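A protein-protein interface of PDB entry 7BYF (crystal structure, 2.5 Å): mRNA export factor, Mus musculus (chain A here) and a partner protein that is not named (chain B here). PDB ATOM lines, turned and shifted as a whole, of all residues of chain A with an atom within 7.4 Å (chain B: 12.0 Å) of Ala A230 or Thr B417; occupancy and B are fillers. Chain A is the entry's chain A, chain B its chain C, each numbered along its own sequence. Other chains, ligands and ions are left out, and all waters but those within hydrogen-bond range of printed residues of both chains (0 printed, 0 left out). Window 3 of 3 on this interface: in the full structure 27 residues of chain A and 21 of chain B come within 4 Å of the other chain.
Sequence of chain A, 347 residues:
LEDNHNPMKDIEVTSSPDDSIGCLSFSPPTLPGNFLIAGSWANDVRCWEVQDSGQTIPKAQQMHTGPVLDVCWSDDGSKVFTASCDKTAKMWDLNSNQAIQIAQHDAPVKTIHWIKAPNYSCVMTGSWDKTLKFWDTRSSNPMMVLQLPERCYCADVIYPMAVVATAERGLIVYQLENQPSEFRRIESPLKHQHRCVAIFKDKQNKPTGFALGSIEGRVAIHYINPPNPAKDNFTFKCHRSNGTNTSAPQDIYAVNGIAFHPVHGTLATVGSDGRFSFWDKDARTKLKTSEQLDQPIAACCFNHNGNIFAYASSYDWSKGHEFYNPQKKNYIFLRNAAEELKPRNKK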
ATOM      1  N   PRO A 226       9.002  10.332  -8.780  1.00  0.00           N
ATOM      2  CA  PRO A 226      10.018  10.054  -7.761  1.00  0.00           C
ATOM      3  C   PRO A 226      11.259   9.434  -8.373  1.00  0.00           C
ATOM      4  O   PRO A 226      11.172   8.669  -9.353  1.00  0.00           O
ATOM      5  CB  PRO A 226       9.307   9.063  -6.822  1.00  0.00           C
ATOM      6  CG  PRO A 226       8.386   8.312  -7.746  1.00  0.00           C
ATOM      7  CD  PRO A 226       7.914   9.329  -8.757  1.00  0.00           C
ATOM      8  N   PRO A 227      12.451   9.736  -7.837  1.00  0.00           N
ATOM      9  CA  PRO A 227      13.657   9.024  -8.296  1.00  0.00           C
ATOM     10  C   PRO A 227      13.542   7.509  -8.220  1.00  0.00           C
ATOM     11  O   PRO A 227      14.026   6.816  -9.123  1.00  0.00           O
ATOM     12  CB  PRO A 227      14.742   9.570  -7.362  1.00  0.00           C
ATOM     13  CG  PRO A 227      14.292  10.971  -7.090  1.00  0.00           C
ATOM     14  CD  PRO A 227      12.788  10.908  -7.009  1.00  0.00           C
ATOM     15  N   ASN A 228      12.888   6.975  -7.188  1.00  0.00           N
ATOM     16  CA  ASN A 228      12.802   5.530  -6.973  1.00  0.00           C
ATOM     17  C   ASN A 228      11.389   5.180  -6.513  1.00  0.00           C
ATOM     18  O   ASN A 228      11.101   5.132  -5.310  1.00  0.00           O
ATOM     19  CB  ASN A 228      13.856   5.075  -5.958  1.00  0.00           C
ATOM     20  CG  ASN A 228      14.053   3.569  -5.942  1.00  0.00           C
ATOM     21  OD1 ASN A 228      13.223   2.815  -6.460  1.00  0.00           O
ATOM     22  ND2 ASN A 228      15.150   3.119  -5.328  1.00  0.00           N
ATOM     23  N   PRO A 229      10.470   4.947  -7.458  1.00  0.00           N
ATOM     24  CA  PRO A 229       9.090   4.586  -7.085  1.00  0.00           C
ATOM     25  C   PRO A 229       8.956   3.428  -6.104  1.00  0.00           C
ATOM     26  O   PRO A 229       8.163   3.540  -5.163  1.00  0.00           O
ATOM     27  CB  PRO A 229       8.459   4.250  -8.444  1.00  0.00           C
ATOM     28  CG  PRO A 229       9.135   5.182  -9.376  1.00  0.00           C
ATOM     29  CD  PRO A 229      10.572   5.271  -8.892  1.00  0.00           C
ATOM     30  N   ALA A 230       9.687   2.323  -6.286  1.00  0.00           N
ATOM     31  CA  ALA A 230       9.483   1.174  -5.407  1.00  0.00           C
ATOM     32  C   ALA A 230       9.825   1.486  -3.961  1.00  0.00           C
ATOM     33  O   ALA A 230       9.376   0.764  -3.067  1.00  0.00           O
ATOM     34  CB  ALA A 230      10.310  -0.021  -5.863  1.00  0.00           C
ATOM     35  N   LYS A 231      10.611   2.537  -3.716  1.00  0.00           N
ATOM     36  CA  LYS A 231      11.011   2.940  -2.375  1.00  0.00           C
ATOM     37  C   LYS A 231      10.402   4.259  -1.922  1.00  0.00           C
ATOM     38  O   LYS A 231      10.097   4.408  -0.740  1.00  0.00           O
ATOM     39  CB  LYS A 231      12.541   3.041  -2.286  1.00  0.00           C
ATOM     40  CG  LYS A 231      13.261   1.685  -2.218  1.00  0.00           C
ATOM     41  CD  LYS A 231      14.791   1.822  -2.339  1.00  0.00           C
ATOM     42  CE  LYS A 231      15.429   2.566  -1.158  1.00  0.00           C
ATOM     43  NZ  LYS A 231      15.725   1.680   0.007  1.00  0.00           N
ATOM     44  N   ASP A 232      10.194   5.206  -2.831  1.00  0.00           N
ATOM     45  CA  ASP A 232       9.742   6.541  -2.455  1.00  0.00           C
ATOM     46  C   ASP A 232       8.227   6.671  -2.312  1.00  0.00           C
ATOM     47  O   ASP A 232       7.760   7.606  -1.641  1.00  0.00           O
ATOM     48  CB  ASP A 232      10.246   7.556  -3.480  1.00  0.00           C
ATOM     49  CG  ASP A 232      11.746   7.594  -3.543  1.00  0.00           C
ATOM     50  OD1 ASP A 232      12.384   7.402  -2.480  1.00  0.00           O
ATOM     51  OD2 ASP A 232      12.286   7.802  -4.650  1.00  0.00           O
ATOM     52  N   ASN A 233       7.453   5.792  -2.941  1.00  0.00           N
ATOM     53  CA  ASN A 233       6.016   5.750  -2.741  1.00  0.00           C
ATOM     54  C   ASN A 233       5.712   4.677  -1.715  1.00  0.00           C
ATOM     55  O   ASN A 233       6.153   3.532  -1.858  1.00  0.00           O
ATOM     56  CB  ASN A 233       5.285   5.488  -4.053  1.00  0.00           C
ATOM     57  CG  ASN A 233       5.463   6.620  -5.036  1.00  0.00           C
ATOM     58  OD1 ASN A 233       5.647   7.768  -4.637  1.00  0.00           O
ATOM     59  ND2 ASN A 233       5.424   6.306  -6.326  1.00  0.00           N
ATOM     60  N   PHE A 234       4.986   5.062  -0.669  1.00  0.00           N
ATOM     61  CA  PHE A 234       4.718   4.188   0.464  1.00  0.00           C
ATOM     62  C   PHE A 234       3.339   4.506   1.025  1.00  0.00           C
ATOM     63  O   PHE A 234       2.709   5.505   0.664  1.00  0.00           O
ATOM     64  CB  PHE A 234       5.797   4.335   1.542  1.00  0.00           C
ATOM     65  CG  PHE A 234       5.859   5.708   2.185  1.00  0.00           C
ATOM     66  CD1 PHE A 234       6.467   6.778   1.532  1.00  0.00           C
ATOM     67  CD2 PHE A 234       5.349   5.915   3.463  1.00  0.00           C
ATOM     68  CE1 PHE A 234       6.548   8.044   2.138  1.00  0.00           C
ATOM     69  CE2 PHE A 234       5.422   7.170   4.075  1.00  0.00           C
ATOM     70  CZ  PHE A 234       6.024   8.241   3.412  1.00  0.00           C
ATOM     71  N   THR A 235       2.868   3.636   1.913  1.00  0.00           N
ATOM     72  CA  THR A 235       1.653   3.877   2.678  1.00  0.00           C
ATOM     73  C   THR A 235       1.993   3.877   4.167  1.00  0.00           C
ATOM     74  O   THR A 235       3.114   3.548   4.562  1.00  0.00           O
ATOM     75  CB  THR A 235       0.563   2.836   2.348  1.00  0.00           C
ATOM     76  OG1 THR A 235       0.896   1.556   2.910  1.00  0.00           O
ATOM     77  CG2 THR A 235       0.386   2.712   0.832  1.00  0.00           C
ATOM     78  N   ARG A 284       9.095  10.345   7.864  1.00  0.00           N
ATOM     79  CA  ARG A 284       8.223   9.181   8.042  1.00  0.00           C
ATOM     80  C   ARG A 284       7.941   8.947   9.521  1.00  0.00           C
ATOM     81  O   ARG A 284       8.024   7.829  10.037  1.00  0.00           O
ATOM     82  CB  ARG A 284       8.811   7.941   7.374  1.00  0.00           C
ATOM     83  CG  ARG A 284       9.025   8.137   5.897  1.00  0.00           C
ATOM     84  CD  ARG A 284       9.211   6.819   5.171  1.00  0.00           C
ATOM     85  NE  ARG A 284       9.505   7.065   3.767  1.00  0.00           N
ATOM     86  CZ  ARG A 284       9.712   6.119   2.865  1.00  0.00           C
ATOM     87  NH1 ARG A 284       9.661   4.840   3.222  1.00  0.00           N
ATOM     88  NH2 ARG A 284       9.975   6.462   1.606  1.00  0.00           N
ATOM     89  N   MET B 413       6.371   6.499  11.749  1.00  0.00           N
ATOM     90  CA  MET B 413       5.300   5.849  11.002  1.00  0.00           C
ATOM     91  C   MET B 413       5.533   4.344  10.968  1.00  0.00           C
ATOM     92  O   MET B 413       6.678   3.889  10.910  1.00  0.00           O
ATOM     93  CB  MET B 413       5.260   6.380   9.563  1.00  0.00           C
ATOM     94  CG  MET B 413       4.705   7.749   9.417  1.00  0.00           C
ATOM     95  SD  MET B 413       4.756   8.199   7.680  1.00  0.00           S
ATOM     96  CE  MET B 413       3.960   9.800   7.728  1.00  0.00           C
ATOM     97  N   GLU B 414       4.464   3.561  10.989  1.00  0.00           N
ATOM     98  CA  GLU B 414       4.603   2.166  10.609  1.00  0.00           C
ATOM     99  C   GLU B 414       4.122   2.061   9.164  1.00  0.00           C
ATOM    100  O   GLU B 414       2.920   2.083   8.875  1.00  0.00           O
ATOM    101  CB  GLU B 414       3.892   1.224  11.574  1.00  0.00           C
ATOM    102  CG  GLU B 414       2.427   1.380  11.742  1.00  0.00           C
ATOM    103  CD  GLU B 414       1.868   0.259  12.588  1.00  0.00           C
ATOM    104  OE1 GLU B 414       1.527   0.521  13.766  1.00  0.00           O
ATOM    105  OE2 GLU B 414       1.806  -0.886  12.076  1.00  0.00           O
ATOM    106  N   TRP B 415       5.084   1.974   8.254  1.00  0.00           N
ATOM    107  CA  TRP B 415       4.836   2.184   6.842  1.00  0.00           C
ATOM    108  C   TRP B 415       5.234   0.958   6.032  1.00  0.00           C
ATOM    109  O   TRP B 415       6.039   0.127   6.463  1.00  0.00           O
ATOM    110  CB  TRP B 415       5.579   3.428   6.344  1.00  0.00           C
ATOM    111  CG  TRP B 415       7.041   3.441   6.621  1.00  0.00           C
ATOM    112  CD1 TRP B 415       7.671   4.034   7.675  1.00  0.00           C
ATOM    113  CD2 TRP B 415       8.072   2.861   5.812  1.00  0.00           C
ATOM    114  NE1 TRP B 415       9.031   3.847   7.583  1.00  0.00           N
ATOM    115  CE2 TRP B 415       9.304   3.128   6.450  1.00  0.00           C
ATOM    116  CE3 TRP B 415       8.073   2.132   4.615  1.00  0.00           C
ATOM    117  CZ2 TRP B 415      10.526   2.694   5.930  1.00  0.00           C
ATOM    118  CZ3 TRP B 415       9.290   1.701   4.099  1.00  0.00           C
ATOM    119  CH2 TRP B 415      10.497   1.987   4.754  1.00  0.00           C
ATOM    120  N   GLN B 416       4.642   0.862   4.846  1.00  0.00           N
ATOM    121  CA  GLN B 416       4.804  -0.261   3.937  1.00  0.00           C
ATOM    122  C   GLN B 416       5.072   0.293   2.540  1.00  0.00           C
ATOM    123  O   GLN B 416       4.889   1.487   2.281  1.00  0.00           O
ATOM    124  CB  GLN B 416       3.547  -1.175   3.937  1.00  0.00           C
ATOM    125  CG  GLN B 416       3.072  -1.700   5.339  1.00  0.00           C
ATOM    126  CD  GLN B 416       2.274  -0.662   6.190  1.00  0.00           C
ATOM    127  OE1 GLN B 416       1.337  -0.010   5.694  1.00  0.00           O
ATOM    128  NE2 GLN B 416       2.641  -0.531   7.478  1.00  0.00           N
ATOM    129  N   THR B 417       5.535  -0.575   1.636  1.00  0.00           N
ATOM    130  CA  THR B 417       5.633  -0.250   0.217  1.00  0.00           C
ATOM    131  C   THR B 417       5.023  -1.392  -0.582  1.00  0.00           C
ATOM    132  O   THR B 417       4.742  -2.469  -0.052  1.00  0.00           O
ATOM    133  CB  THR B 417       7.079  -0.017  -0.249  1.00  0.00           C
ATOM    134  OG1 THR B 417       7.846  -1.214  -0.054  1.00  0.00           O
ATOM    135  CG2 THR B 417       7.735   1.192   0.472  1.00  0.00           C
ATOM    136  N   LEU B 418       4.838  -1.136  -1.876  1.00  0.00           N
ATOM    137  CA  LEU B 418       4.202  -2.086  -2.794  1.00  0.00           C
ATOM    138  C   LEU B 418       5.122  -3.268  -3.092  1.00  0.00           C
ATOM    139  O   LEU B 418       5.573  -3.966  -2.181  1.00  0.00           O
ATOM    140  CB  LEU B 418       3.798  -1.383  -4.106  1.00  0.00           C
ATOM    141  CG  LEU B 418       2.958  -0.090  -4.048  1.00  0.00           C
ATOM    142  CD1 LEU B 418       2.713   0.472  -5.459  1.00  0.00           C
ATOM    143  CD2 LEU B 418       1.632  -0.249  -3.255  1.00  0.00           C
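Of the 11 printed residues of chain A, 5 touch a printed residue of chain B. Hydrophobic or aromatic side chains of chain A that line the printed part of chain B: Phe A234. Hydrophobic or aromatic side chains of chain B that line the printed part of chain A: Met B413 and Trp B415.
CB of Thr B417 touches O of Ala A230, 3.7 Å away. Thr B417 touches Asn A233 (CG2 to O, 3.7 Å). Met B413 touches Phe A234 (SD to CE2, 3.8 Å). Trp B415 touches Phe A234. Phe A234 touches Gln B416. Phe A234 touches Thr B417. O of Thr A235 touches CB of Trp B415, at 3.0 Å. Arg A284 touches Trp B415 (NH1 to CZ3, 3.3 Å).
The backbone NH of Thr A235 is in hydrogen-bond range of the backbone carbonyl oxygen of Gln B416, 3.0 Å away. The backbone NH of Met B413 lies within hydrogen-bond range of the backbone carbonyl oxygen of Arg A284 (2.7 Å).
The backbone carbonyl oxygen (O) of Glu B414 is in hydrogen-bond range of the side-chain amide nitrogen (NE2) of Gln B416, 3.0 Å away. The backbone carbonyl oxygen of Lys A231 is in hydrogen-bond range of the guanidinium group of Arg A284, 3.1 Å away.
Of chain B, only Thr B417 (3.7 Å) comes within 4 Å of Ala A230. Of the printed residues of chain A, Thr B417 touches Ala A230 (3.7 Å), Asn A233 (3.7 Å) and Phe A234 (3.8 Å). No residue of chain B comes within 4 Å of Asn A228. No residue of chain B comes within 4 Å of Pro A229. Of the printed residues of chain B, Asn A233 touches Thr B417 (3.7 Å). Phe A234 touches just these residues of chain B: Met B413, Trp B415, Gln B416 and Thr B417. Of chain B, only Trp B415 and Gln B416 come within 4 Å of Thr A235. Printed residues of chain A within 4 Å of Gln B416: Phe A234 and Thr A235. Of the printed residues of chain A, Met B413 touches Phe A234 and Arg A284. Of the printed residues of chain B, Arg A284 touches Met B413 (2.7 Å) and Trp B415 (3.3 Å). Of the printed residues of chain A, Trp B415 touches Phe A234 (3.8 Å), Thr A235 (3.0 Å) and Arg A284 (3.3 Å). Leu B418 touches none of the printed residues of chain A. Pro A227 touches none of the printed residues of chain B. The nearest residue of chain B that does not touch Ala A230 is Leu B418 (5.1 Å). The nearest residue of chain A that does not touch Thr B417 is Lys A231 (4.2 Å). The nearest printed residue of chain A that does not touch Trp B415 is Lys A231 (5.6 Å).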
